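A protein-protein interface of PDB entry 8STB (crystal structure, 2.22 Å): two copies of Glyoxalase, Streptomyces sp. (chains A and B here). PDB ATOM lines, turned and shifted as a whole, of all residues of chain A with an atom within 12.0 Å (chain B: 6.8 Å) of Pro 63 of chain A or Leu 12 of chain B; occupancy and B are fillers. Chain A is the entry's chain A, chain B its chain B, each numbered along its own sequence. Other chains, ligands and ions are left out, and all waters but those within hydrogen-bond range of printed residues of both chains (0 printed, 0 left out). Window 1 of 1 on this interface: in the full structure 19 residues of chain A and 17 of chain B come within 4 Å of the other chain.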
ATOM      1  N   LEU A  12     -27.021 -20.595 -11.851  1.00  0.00           N
ATOM      2  CA  LEU A  12     -26.238 -19.807 -12.795  1.00  0.00           C
ATOM      3  C   LEU A  12     -25.428 -18.791 -12.009  1.00  0.00           C
ATOM      4  O   LEU A  12     -26.003 -17.981 -11.267  1.00  0.00           O
ATOM      5  CB  LEU A  12     -27.134 -19.095 -13.796  1.00  0.00           C
ATOM      6  CG  LEU A  12     -27.888 -19.993 -14.785  1.00  0.00           C
ATOM      7  CD1 LEU A  12     -28.602 -19.061 -15.794  1.00  0.00           C
ATOM      8  CD2 LEU A  12     -27.052 -21.023 -15.468  1.00  0.00           C
ATOM      9  N   PRO A  14     -21.618 -16.306 -11.963  1.00  0.00           N
ATOM     10  CA  PRO A  14     -20.471 -15.763 -12.732  1.00  0.00           C
ATOM     11  C   PRO A  14     -19.136 -16.232 -12.158  1.00  0.00           C
ATOM     12  O   PRO A  14     -18.117 -15.828 -12.759  1.00  0.00           O
ATOM     13  CB  PRO A  14     -20.679 -14.258 -12.632  1.00  0.00           C
ATOM     14  CG  PRO A  14     -21.240 -14.106 -11.235  1.00  0.00           C
ATOM     15  CD  PRO A  14     -22.196 -15.234 -11.096  1.00  0.00           C
ATOM     16  N   ASP A  56     -22.254 -21.216 -15.996  1.00  0.00           N
ATOM     17  CA  ASP A  56     -21.631 -19.865 -16.046  1.00  0.00           C
ATOM     18  C   ASP A  56     -22.589 -18.788 -16.554  1.00  0.00           C
ATOM     19  O   ASP A  56     -23.081 -18.931 -17.691  1.00  0.00           O
ATOM     20  CB  ASP A  56     -20.410 -19.870 -16.951  1.00  0.00           C
ATOM     21  CG  ASP A  56     -19.146 -20.465 -16.351  1.00  0.00           C
ATOM     22  OD1 ASP A  56     -18.882 -20.221 -15.156  1.00  0.00           O
ATOM     23  OD2 ASP A  56     -18.425 -21.158 -17.091  1.00  0.00           O
ATOM     24  N   LEU A  57     -22.831 -17.749 -15.755  1.00  0.00           N
ATOM     25  CA  LEU A  57     -23.634 -16.570 -16.176  1.00  0.00           C
ATOM     26  C   LEU A  57     -22.875 -15.876 -17.312  1.00  0.00           C
ATOM     27  O   LEU A  57     -23.533 -15.395 -18.254  1.00  0.00           O
ATOM     28  CB  LEU A  57     -23.799 -15.646 -14.970  1.00  0.00           C
ATOM     29  CG  LEU A  57     -24.537 -14.325 -15.201  1.00  0.00           C
ATOM     30  CD1 LEU A  57     -25.968 -14.606 -15.621  1.00  0.00           C
ATOM     31  CD2 LEU A  57     -24.500 -13.464 -13.958  1.00  0.00           C
ATOM     32  N   GLY A  58     -21.548 -15.843 -17.227  1.00  0.00           N
ATOM     33  CA  GLY A  58     -20.654 -15.153 -18.182  1.00  0.00           C
ATOM     34  C   GLY A  58     -20.702 -15.691 -19.597  1.00  0.00           C
ATOM     35  O   GLY A  58     -20.520 -14.873 -20.519  1.00  0.00           O
ATOM     36  N   GLU A  59     -20.924 -16.986 -19.809  1.00  0.00           N
ATOM     37  CA  GLU A  59     -20.741 -17.607 -21.147  1.00  0.00           C
ATOM     38  C   GLU A  59     -21.617 -16.983 -22.246  1.00  0.00           C
ATOM     39  O   GLU A  59     -21.086 -16.837 -23.364  1.00  0.00           O
ATOM     40  CB  GLU A  59     -21.109 -19.086 -21.061  1.00  0.00           C
ATOM     41  CG  GLU A  59     -19.967 -20.014 -21.458  1.00  0.00           C
ATOM     42  CD  GLU A  59     -19.038 -20.359 -20.311  1.00  0.00           C
ATOM     43  OE1 GLU A  59     -18.893 -21.565 -20.024  1.00  0.00           O
ATOM     44  OE2 GLU A  59     -18.465 -19.429 -19.707  1.00  0.00           O
ATOM     45  N   ASN A  60     -22.876 -16.644 -21.971  1.00  0.00           N
ATOM     46  CA  ASN A  60     -23.788 -16.033 -22.979  1.00  0.00           C
ATOM     47  C   ASN A  60     -23.901 -14.524 -22.729  1.00  0.00           C
ATOM     48  O   ASN A  60     -23.724 -14.118 -21.561  1.00  0.00           O
ATOM     49  CB  ASN A  60     -25.137 -16.736 -22.968  1.00  0.00           C
ATOM     50  CG  ASN A  60     -24.979 -18.229 -23.115  1.00  0.00           C
ATOM     51  OD1 ASN A  60     -24.945 -18.743 -24.238  1.00  0.00           O
ATOM     52  ND2 ASN A  60     -24.861 -18.935 -22.002  1.00  0.00           N
ATOM     53  N   PRO A  61     -24.184 -13.676 -23.750  1.00  0.00           N
ATOM     54  CA  PRO A  61     -24.382 -12.214 -23.557  1.00  0.00           C
ATOM     55  C   PRO A  61     -25.838 -11.875 -23.281  1.00  0.00           C
ATOM     56  O   PRO A  61     -26.615 -12.801 -22.962  1.00  0.00           O
ATOM     57  CB  PRO A  61     -23.913 -11.667 -24.895  1.00  0.00           C
ATOM     58  CG  PRO A  61     -24.532 -12.665 -25.856  1.00  0.00           C
ATOM     59  CD  PRO A  61     -24.355 -14.005 -25.204  1.00  0.00           C
ATOM     60  N   GLY A  62     -26.197 -10.590 -23.358  1.00  0.00           N
ATOM     61  CA  GLY A  62     -27.591 -10.133 -23.207  1.00  0.00           C
ATOM     62  C   GLY A  62     -27.958  -9.983 -21.755  1.00  0.00           C
ATOM     63  O   GLY A  62     -27.105 -10.284 -20.896  1.00  0.00           O
ATOM     64  N   PRO A  63     -29.181  -9.531 -21.421  1.00  0.00           N
ATOM     65  CA  PRO A  63     -29.621  -9.486 -20.006  1.00  0.00           C
ATOM     66  C   PRO A  63     -29.693 -10.921 -19.510  1.00  0.00           C
ATOM     67  O   PRO A  63     -30.139 -11.787 -20.295  1.00  0.00           O
ATOM     68  CB  PRO A  63     -30.947  -8.743 -20.030  1.00  0.00           C
ATOM     69  CG  PRO A  63     -31.412  -8.711 -21.471  1.00  0.00           C
ATOM     70  CD  PRO A  63     -30.232  -9.003 -22.342  1.00  0.00           C
ATOM     71  N   ALA A  64     -29.277 -11.178 -18.273  1.00  0.00           N
ATOM     72  CA  ALA A  64     -29.239 -12.545 -17.708  1.00  0.00           C
ATOM     73  C   ALA A  64     -29.365 -12.474 -16.191  1.00  0.00           C
ATOM     74  O   ALA A  64     -28.700 -11.610 -15.598  1.00  0.00           O
ATOM     75  CB  ALA A  64     -27.958 -13.225 -18.112  1.00  0.00           C
ATOM     76  N   LEU A  65     -30.183 -13.340 -15.591  1.00  0.00           N
ATOM     77  CA  LEU A  65     -30.369 -13.370 -14.153  1.00  0.00           C
ATOM     78  C   LEU A  65     -29.725 -14.624 -13.592  1.00  0.00           C
ATOM     79  O   LEU A  65     -30.074 -15.742 -13.986  1.00  0.00           O
ATOM     80  CB  LEU A  65     -31.850 -13.338 -13.819  1.00  0.00           C
ATOM     81  CG  LEU A  65     -32.513 -11.983 -14.079  1.00  0.00           C
ATOM     82  CD1 LEU A  65     -34.009 -12.038 -13.794  1.00  0.00           C
ATOM     83  CD2 LEU A  65     -31.829 -10.908 -13.229  1.00  0.00           C
ATOM     84  N   GLY A  66     -28.762 -14.425 -12.697  1.00  0.00           N
ATOM     85  CA  GLY A  66     -28.111 -15.501 -11.982  1.00  0.00           C
ATOM     86  C   GLY A  66     -28.954 -15.961 -10.806  1.00  0.00           C
ATOM     87  O   GLY A  66     -30.038 -15.429 -10.532  1.00  0.00           O
ATOM     88  N   GLY A  67     -28.464 -16.991 -10.115  1.00  0.00           N
ATOM     89  CA  GLY A  67     -29.194 -17.531  -8.989  1.00  0.00           C
ATOM     90  C   GLY A  67     -29.670 -18.949  -9.259  1.00  0.00           C
ATOM     91  O   GLY A  67     -29.406 -19.548 -10.309  1.00  0.00           O
ATOM     92  N   SER A  69     -32.484 -21.596 -10.000  1.00  0.00           N
ATOM     93  CA  SER A  69     -33.759 -21.758 -10.690  1.00  0.00           C
ATOM     94  C   SER A  69     -34.383 -23.093 -10.321  1.00  0.00           C
ATOM     95  O   SER A  69     -33.713 -24.128 -10.379  1.00  0.00           O
ATOM     96  CB  SER A  69     -33.569 -21.700 -12.205  1.00  0.00           C
ATOM     97  OG  SER A  69     -33.162 -20.417 -12.623  1.00  0.00           O
ATOM     98  N   LEU A  92     -42.302 -15.854 -19.600  1.00  0.00           N
ATOM     99  CA  LEU A  92     -41.033 -15.141 -19.755  1.00  0.00           C
ATOM    100  C   LEU A  92     -40.116 -15.780 -20.802  1.00  0.00           C
ATOM    101  O   LEU A  92     -39.311 -15.080 -21.431  1.00  0.00           O
ATOM    102  CB  LEU A  92     -40.294 -15.099 -18.404  1.00  0.00           C
ATOM    103  CG  LEU A  92     -41.173 -14.731 -17.205  1.00  0.00           C
ATOM    104  CD1 LEU A  92     -40.515 -14.759 -15.877  1.00  0.00           C
ATOM    105  CD2 LEU A  92     -41.731 -13.321 -17.485  1.00  0.00           C
ATOM    106  N   LEU A  93     -40.229 -17.092 -21.007  1.00  0.00           N
ATOM    107  CA  LEU A  93     -39.437 -17.808 -21.998  1.00  0.00           C
ATOM    108  C   LEU A  93     -40.128 -19.120 -22.328  1.00  0.00           C
ATOM    109  O   LEU A  93     -40.614 -19.805 -21.424  1.00  0.00           O
ATOM    110  CB  LEU A  93     -38.024 -18.082 -21.481  1.00  0.00           C
ATOM    111  CG  LEU A  93     -37.071 -18.741 -22.493  1.00  0.00           C
ATOM    112  CD1 LEU A  93     -36.605 -17.788 -23.554  1.00  0.00           C
ATOM    113  CD2 LEU A  93     -35.868 -19.334 -21.742  1.00  0.00           C
ATOM    114  N   LEU A 106     -40.378 -20.744 -18.885  1.00  0.00           N
ATOM    115  CA  LEU A 106     -40.201 -19.977 -17.656  1.00  0.00           C
ATOM    116  C   LEU A 106     -41.395 -19.048 -17.482  1.00  0.00           C
ATOM    117  O   LEU A 106     -41.812 -18.391 -18.432  1.00  0.00           O
ATOM    118  CB  LEU A 106     -38.902 -19.171 -17.683  1.00  0.00           C
ATOM    119  CG  LEU A 106     -37.614 -19.945 -17.967  1.00  0.00           C
ATOM    120  CD1 LEU A 106     -36.451 -18.911 -17.905  1.00  0.00           C
ATOM    121  CD2 LEU A 106     -37.342 -21.078 -17.009  1.00  0.00           C
ATOM    122  N   ARG A 114     -40.357 -15.860 -10.388  1.00  0.00           N
ATOM    123  CA  ARG A 114     -40.028 -16.654 -11.567  1.00  0.00           C
ATOM    124  C   ARG A 114     -39.931 -18.126 -11.205  1.00  0.00           C
ATOM    125  O   ARG A 114     -39.384 -18.492 -10.154  1.00  0.00           O
ATOM    126  CB  ARG A 114     -38.698 -16.212 -12.197  1.00  0.00           C
ATOM    127  CG  ARG A 114     -38.654 -14.747 -12.672  1.00  0.00           C
ATOM    128  CD  ARG A 114     -37.238 -14.369 -13.164  1.00  0.00           C
ATOM    129  NE  ARG A 114     -36.321 -14.113 -12.050  1.00  0.00           N
ATOM    130  CZ  ARG A 114     -36.281 -12.970 -11.371  1.00  0.00           C
ATOM    131  NH1 ARG A 114     -37.071 -11.961 -11.679  1.00  0.00           N
ATOM    132  NH2 ARG A 114     -35.433 -12.836 -10.353  1.00  0.00           N
ATOM    133  N   ASP B  10     -31.892  -1.857 -26.525  1.00  0.00           N
ATOM    134  CA  ASP B  10     -32.367  -1.616 -25.171  1.00  0.00           C
ATOM    135  C   ASP B  10     -31.368  -2.245 -24.214  1.00  0.00           C
ATOM    136  O   ASP B  10     -30.920  -3.367 -24.436  1.00  0.00           O
ATOM    137  CB  ASP B  10     -33.777  -2.231 -25.034  1.00  0.00           C
ATOM    138  CG  ASP B  10     -34.416  -1.957 -23.739  1.00  0.00           C
ATOM    139  OD1 ASP B  10     -34.347  -0.797 -23.268  1.00  0.00           O
ATOM    140  OD2 ASP B  10     -35.035  -2.895 -23.191  1.00  0.00           O
ATOM    141  N   LEU B  11     -31.008  -1.536 -23.166  1.00  0.00           N
ATOM    142  CA  LEU B  11     -30.069  -2.059 -22.190  1.00  0.00           C
ATOM    143  C   LEU B  11     -30.869  -2.451 -20.954  1.00  0.00           C
ATOM    144  O   LEU B  11     -31.591  -1.622 -20.387  1.00  0.00           O
ATOM    145  CB  LEU B  11     -28.978  -1.036 -21.851  1.00  0.00           C
ATOM    146  CG  LEU B  11     -28.143  -1.469 -20.649  1.00  0.00           C
ATOM    147  CD1 LEU B  11     -27.405  -2.809 -20.884  1.00  0.00           C
ATOM    148  CD2 LEU B  11     -27.113  -0.391 -20.261  1.00  0.00           C
ATOM    149  N   LEU B  12     -30.740  -3.705 -20.532  1.00  0.00           N
ATOM    150  CA  LEU B  12     -31.255  -4.141 -19.236  1.00  0.00           C
ATOM    151  C   LEU B  12     -30.066  -4.381 -18.321  1.00  0.00           C
ATOM    152  O   LEU B  12     -29.174  -5.164 -18.656  1.00  0.00           O
ATOM    153  CB  LEU B  12     -32.140  -5.379 -19.363  1.00  0.00           C
ATOM    154  CG  LEU B  12     -33.510  -5.129 -19.974  1.00  0.00           C
ATOM    155  CD1 LEU B  12     -34.333  -6.411 -20.032  1.00  0.00           C
ATOM    156  CD2 LEU B  12     -34.269  -4.105 -19.133  1.00  0.00           C
ATOM    157  N   THR B  13     -30.049  -3.695 -17.182  1.00  0.00           N
ATOM    158  CA  THR B  13     -28.886  -3.650 -16.312  1.00  0.00           C
ATOM    159  C   THR B  13     -29.322  -3.776 -14.863  1.00  0.00           C
ATOM    160  O   THR B  13     -30.408  -3.303 -14.487  1.00  0.00           O
ATOM    161  CB  THR B  13     -28.078  -2.344 -16.515  1.00  0.00           C
ATOM    162  OG1 THR B  13     -26.995  -2.277 -15.584  1.00  0.00           O
ATOM    163  CG2 THR B  13     -28.937  -1.120 -16.294  1.00  0.00           C
ATOM    164  N   PRO B  14     -28.495  -4.405 -14.019  1.00  0.00           N
ATOM    165  CA  PRO B  14     -28.814  -4.431 -12.584  1.00  0.00           C
ATOM    166  C   PRO B  14     -28.508  -3.133 -11.863  1.00  0.00           C
ATOM    167  O   PRO B  14     -28.863  -3.020 -10.691  1.00  0.00           O
ATOM    168  CB  PRO B  14     -27.936  -5.571 -12.035  1.00  0.00           C
ATOM    169  CG  PRO B  14     -26.730  -5.583 -12.995  1.00  0.00           C
ATOM    170  CD  PRO B  14     -27.280  -5.184 -14.355  1.00  0.00           C
ATOM    171  N   ASP B  15     -27.862  -2.148 -12.508  1.00  0.00           N
ATOM    172  CA  ASP B  15     -27.551  -0.845 -11.866  1.00  0.00           C
ATOM    173  C   ASP B  15     -27.759   0.270 -12.893  1.00  0.00           C
ATOM    174  O   ASP B  15     -26.816   0.730 -13.555  1.00  0.00           O
ATOM    175  CB  ASP B  15     -26.136  -0.828 -11.289  1.00  0.00           C
ATOM    176  CG  ASP B  15     -25.877   0.396 -10.395  1.00  0.00           C
ATOM    177  OD1 ASP B  15     -26.690   1.367 -10.417  1.00  0.00           O
ATOM    178  OD2 ASP B  15     -24.869   0.376  -9.647  1.00  0.00           O
ATOM    179  N   PRO B  40     -39.701   2.328 -14.697  1.00  0.00           N
ATOM    180  CA  PRO B  40     -38.830   1.169 -14.936  1.00  0.00           C
ATOM    181  C   PRO B  40     -37.775   1.397 -16.007  1.00  0.00           C
ATOM    182  O   PRO B  40     -36.773   0.667 -16.012  1.00  0.00           O
ATOM    183  CB  PRO B  40     -39.818   0.053 -15.329  1.00  0.00           C
ATOM    184  CG  PRO B  40     -40.966   0.777 -15.931  1.00  0.00           C
ATOM    185  CD  PRO B  40     -41.063   2.114 -15.231  1.00  0.00           C
ATOM    186  N   SER B  53     -33.028   2.997 -24.959  1.00  0.00           N
ATOM    187  CA  SER B  53     -33.569   3.010 -23.610  1.00  0.00           C
ATOM    188  C   SER B  53     -32.693   2.148 -22.715  1.00  0.00           C
ATOM    189  O   SER B  53     -31.963   1.275 -23.184  1.00  0.00           O
ATOM    190  CB  SER B  53     -35.021   2.497 -23.580  1.00  0.00           C
ATOM    191  OG  SER B  53     -35.110   1.194 -24.150  1.00  0.00           O
ATOM    192  N   ILE B  54     -32.759   2.432 -21.420  1.00  0.00           N
ATOM    193  CA  ILE B  54     -32.048   1.687 -20.393  1.00  0.00           C
ATOM    194  C   ILE B  54     -33.049   1.328 -19.312  1.00  0.00           C
ATOM    195  O   ILE B  54     -33.791   2.199 -18.850  1.00  0.00           O
ATOM    196  CB  ILE B  54     -30.883   2.502 -19.812  1.00  0.00           C
ATOM    197  CG1 ILE B  54     -29.953   2.929 -20.959  1.00  0.00           C
ATOM    198  CG2 ILE B  54     -30.142   1.694 -18.766  1.00  0.00           C
ATOM    199  CD1 ILE B  54     -28.755   3.688 -20.518  1.00  0.00           C
ATOM    200  N   GLY B  55     -33.091   0.040 -18.936  1.00  0.00           N
ATOM    201  CA  GLY B  55     -34.044  -0.447 -17.967  1.00  0.00           C
ATOM    202  C   GLY B  55     -33.382  -1.328 -16.921  1.00  0.00           C
ATOM    203  O   GLY B  55     -32.216  -1.731 -17.042  1.00  0.00           O
ATOM    204  N   ASP B  56     -34.170  -1.648 -15.901  1.00  0.00           N
ATOM    205  CA  ASP B  56     -33.693  -2.432 -14.771  1.00  0.00           C
ATOM    206  C   ASP B  56     -33.911  -3.916 -15.005  1.00  0.00           C
ATOM    207  O   ASP B  56     -34.988  -4.322 -15.428  1.00  0.00           O
ATOM    208  CB  ASP B  56     -34.431  -2.053 -13.486  1.00  0.00           C
ATOM    209  CG  ASP B  56     -34.285  -0.643 -13.138  1.00  0.00           C
ATOM    210  OD1 ASP B  56     -33.139  -0.151 -13.188  1.00  0.00           O
ATOM    211  OD2 ASP B  56     -35.321  -0.024 -12.818  1.00  0.00           O
ATOM    212  N   LEU B  57     -32.875  -4.714 -14.774  1.00  0.00           N
ATOM    213  CA  LEU B  57     -33.071  -6.123 -14.479  1.00  0.00           C
ATOM    214  C   LEU B  57     -33.691  -6.155 -13.090  1.00  0.00           C
ATOM    215  O   LEU B  57     -33.129  -5.575 -12.153  1.00  0.00           O
ATOM    216  CB  LEU B  57     -31.734  -6.842 -14.502  1.00  0.00           C
ATOM    217  CG  LEU B  57     -31.347  -7.497 -15.822  1.00  0.00           C
ATOM    218  CD1 LEU B  57     -30.082  -8.330 -15.556  1.00  0.00           C
ATOM    219  CD2 LEU B  57     -32.417  -8.305 -16.502  1.00  0.00           C
ATOM    220  N   GLY B  58     -34.863  -6.776 -12.952  1.00  0.00           N
ATOM    221  CA  GLY B  58     -35.609  -6.738 -11.679  1.00  0.00           C
ATOM    222  C   GLY B  58     -34.835  -7.251 -10.487  1.00  0.00           C
ATOM    223  O   GLY B  58     -33.794  -7.914 -10.688  1.00  0.00           O
ATOM    224  N   LEU B  65     -26.282 -10.221 -14.881  1.00  0.00           N
ATOM    225  CA  LEU B  65     -25.382  -9.650 -15.910  1.00  0.00           C
ATOM    226  C   LEU B  65     -26.222  -8.866 -16.921  1.00  0.00           C
ATOM    227  O   LEU B  65     -26.903  -9.498 -17.729  1.00  0.00           O
ATOM    228  CB  LEU B  65     -24.641 -10.806 -16.570  1.00  0.00           C
ATOM    229  CG  LEU B  65     -23.919 -10.506 -17.888  1.00  0.00           C
ATOM    230  CD1 LEU B  65     -22.960  -9.335 -17.767  1.00  0.00           C
ATOM    231  CD2 LEU B  65     -23.200 -11.760 -18.343  1.00  0.00           C
ATOM    232  N   GLY B  66     -26.151  -7.540 -16.896  1.00  0.00           N
ATOM    233  CA  GLY B  66     -26.881  -6.697 -17.851  1.00  0.00           C
ATOM    234  C   GLY B  66     -26.355  -6.861 -19.261  1.00  0.00           C
ATOM    235  O   GLY B  66     -25.144  -7.123 -19.390  1.00  0.00           O
ATOM    236  N   GLY B  67     -27.221  -6.816 -20.275  1.00  0.00           N
ATOM    237  CA  GLY B  67     -26.763  -6.836 -21.674  1.00  0.00           C
ATOM    238  C   GLY B  67     -27.642  -6.033 -22.601  1.00  0.00           C
ATOM    239  O   GLY B  67     -28.829  -5.864 -22.277  1.00  0.00           O
ATOM    240  N   TRP B  68     -27.080  -5.522 -23.695  1.00  0.00           N
ATOM    241  CA  TRP B  68     -27.863  -4.832 -24.748  1.00  0.00           C
ATOM    242  C   TRP B  68     -28.706  -5.851 -25.519  1.00  0.00           C
ATOM    243  O   TRP B  68     -28.176  -6.947 -25.791  1.00  0.00           O
ATOM    244  CB  TRP B  68     -26.914  -4.060 -25.671  1.00  0.00           C
ATOM    245  CG  TRP B  68     -26.362  -2.815 -25.034  1.00  0.00           C
ATOM    246  CD1 TRP B  68     -25.181  -2.683 -24.364  1.00  0.00           C
ATOM    247  CD2 TRP B  68     -26.995  -1.520 -24.996  1.00  0.00           C
ATOM    248  NE1 TRP B  68     -25.030  -1.398 -23.920  1.00  0.00           N
ATOM    249  CE2 TRP B  68     -26.125  -0.662 -24.288  1.00  0.00           C
ATOM    250  CE3 TRP B  68     -28.201  -1.007 -25.486  1.00  0.00           C
ATOM    251  CZ2 TRP B  68     -26.428   0.678 -24.066  1.00  0.00           C
ATOM    252  CZ3 TRP B  68     -28.499   0.317 -25.262  1.00  0.00           C
ATOM    253  CH2 TRP B  68     -27.623   1.146 -24.561  1.00  0.00           C
ATOM    254  N   SER B  69     -29.932  -5.494 -25.905  1.00  0.00           N
ATOM    255  CA  SER B  69     -30.863  -6.387 -26.643  1.00  0.00           C
ATOM    256  C   SER B  69     -31.218  -5.720 -27.975  1.00  0.00           C
ATOM    257  O   SER B  69     -31.882  -4.678 -27.928  1.00  0.00           O
ATOM    258  CB  SER B  69     -32.092  -6.691 -25.830  1.00  0.00           C
ATOM    259  OG  SER B  69     -31.821  -7.672 -24.839  1.00  0.00           O
ATOM    260  N   ARG B 114     -29.391 -14.900 -29.674  1.00  0.00           N
ATOM    261  CA  ARG B 114     -30.728 -14.341 -29.512  1.00  0.00           C
ATOM    262  C   ARG B 114     -30.864 -12.970 -30.172  1.00  0.00           C
ATOM    263  O   ARG B 114     -29.923 -12.160 -30.183  1.00  0.00           O
ATOM    264  CB  ARG B 114     -31.095 -14.260 -28.028  1.00  0.00           C
ATOM    265  CG  ARG B 114     -31.100 -15.663 -27.395  1.00  0.00           C
ATOM    266  CD  ARG B 114     -31.387 -15.667 -25.916  1.00  0.00           C
ATOM    267  NE  ARG B 114     -31.526 -17.032 -25.417  1.00  0.00           N
ATOM    268  CZ  ARG B 114     -32.097 -17.346 -24.261  1.00  0.00           C
ATOM    269  NH1 ARG B 114     -32.587 -16.415 -23.459  1.00  0.00           N
ATOM    270  NH2 ARG B 114     -32.189 -18.626 -23.908  1.00  0.00           N
ATOM    271  N   GLU B 227     -21.921  -5.534 -19.744  1.00  0.00           N
ATOM    272  CA  GLU B 227     -22.570  -5.555 -21.040  1.00  0.00           C
ATOM    273  C   GLU B 227     -21.553  -5.144 -22.106  1.00  0.00           C
ATOM    274  O   GLU B 227     -20.587  -4.428 -21.844  1.00  0.00           O
ATOM    275  CB  GLU B 227     -23.780  -4.620 -21.052  1.00  0.00           C
ATOM    276  CG  GLU B 227     -23.474  -3.150 -21.068  1.00  0.00           C
ATOM    277  CD  GLU B 227     -23.331  -2.543 -19.683  1.00  0.00           C
ATOM    278  OE1 GLU B 227     -23.138  -3.299 -18.715  1.00  0.00           O
ATOM    279  OE2 GLU B 227     -23.432  -1.295 -19.574  1.00  0.00           O
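The backbone carbonyl oxygen (O) of Gly 62 of chain A lies close to the backbone carbonyl oxygen (O) of Leu 65 of chain B, 3.3 Å away.
The backbone carbonyl oxygen (O) of Ala 64 of chain A lies within hydrogen-bond range of the backbone NH (N) of Leu 65 of chain B, at 2.9 Å.
O of Leu 12 of chain B sits at hydrogen-bond distance from N of Gly 67 of chain B.
The backbone carbonyl oxygen (O) of Thr 13 of chain B sits at hydrogen-bond distance from the backbone NH (N) of Leu 57 of chain B, 2.9 Å away.
N of Ser 69 of chain B lies within hydrogen-bond range of O of Asp 10 of chain B (2.8 Å).
O of Leu 57 of chain A touches CD2 of Leu 65 of chain B (3.7 Å).
Gly 62 of chain A touches Gly 66 of chain B.
Gly 67 of chain B touches Gly 62 of chain A.
Leu 12 of chain B touches Pro 63 of chain A.
Pro 63 of chain A touches Leu 57 of chain B (CB to CD2, 3.8 Å).
Pro 63 of chain A touches Leu 65 of chain B (CA to O, 3.5 Å).
O of Gly 67 of chain B touches CD of Pro 63 of chain A, at 3.4 Å.
CD of Pro 63 of chain A touches OG of Ser 69 of chain B, at 3.2 Å.
Leu 57 of chain B touches Ala 64 of chain A (CD1 to O, 3.6 Å).
CD2 of Leu 65 of chain A touches CD1 of Leu 57 of chain B, at 3.9 Å.
Of the printed residues of chain B, Gly 62 of chain A touches Leu 65, Gly 66 and Gly 67.
Pro 63 of chain A touches five residues of chain B.
Of the printed residues of chain B, Ala 64 of chain A touches Leu 57 and Leu 65.
Of the printed residues of chain B, Leu 65 of chain A touches Leu 57.
No residue of chain A comes within 4 Å of Leu 11 of chain B.
Of chain A, only Pro 63 (3.6 Å) comes within 4 Å of Leu 12 of chain B.
No residue of chain A comes within 4 Å of Thr 13 of chain B.
Ile 54 of chain B touches none of the printed residues of chain A.
No residue of chain A comes within 4 Å of Asp 56 of chain B.
Leu 65 of chain B touches four residues of chain A.
Of chain A, only Gly 62 comes within 4 Å of Gly 66 of chain B.
Printed residues of chain A within 4 Å of Gly 67 of chain B: Gly 62 and Pro 63.
Printed residues of chain A within 4 Å of Ser 69 of chain B: Pro 63.
The nearest residue of chain B that does not touch Pro 63 of chain A is Gly 66 of chain B (4.3 Å).
The nearest printed residue of chain B that does not touch Leu 57 of chain A is Gly 66 of chain B (6.8 Å).
Of the 19 printed residues of chain A, 5 touch a printed residue of chain B.
Of the 20 printed residues of chain B, 6 touch a printed residue of chain A.
Printed residues of chain B that touch a printed residue of chain A: Leu 12, Leu 57, Leu 65, Gly 66, Gly 67 and Ser 69.
Among the printed residues, no Asp or Glu carboxylate lies within 4 Å of a Lys or Arg side-chain nitrogen of the other chain.
Leu 57 of chain A touches Leu 65 of chain B, and with the chains exchanged Leu 65 of chain A touches Leu 57 of chain B.
Positions printed for both chains: 12, 14, 56, 57, 58, 65, 66, 67, 69 and 114.
Of the 12 pairs that touch across the chains among the printed residues, 2 have their exchanged pair printed and touching as well.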
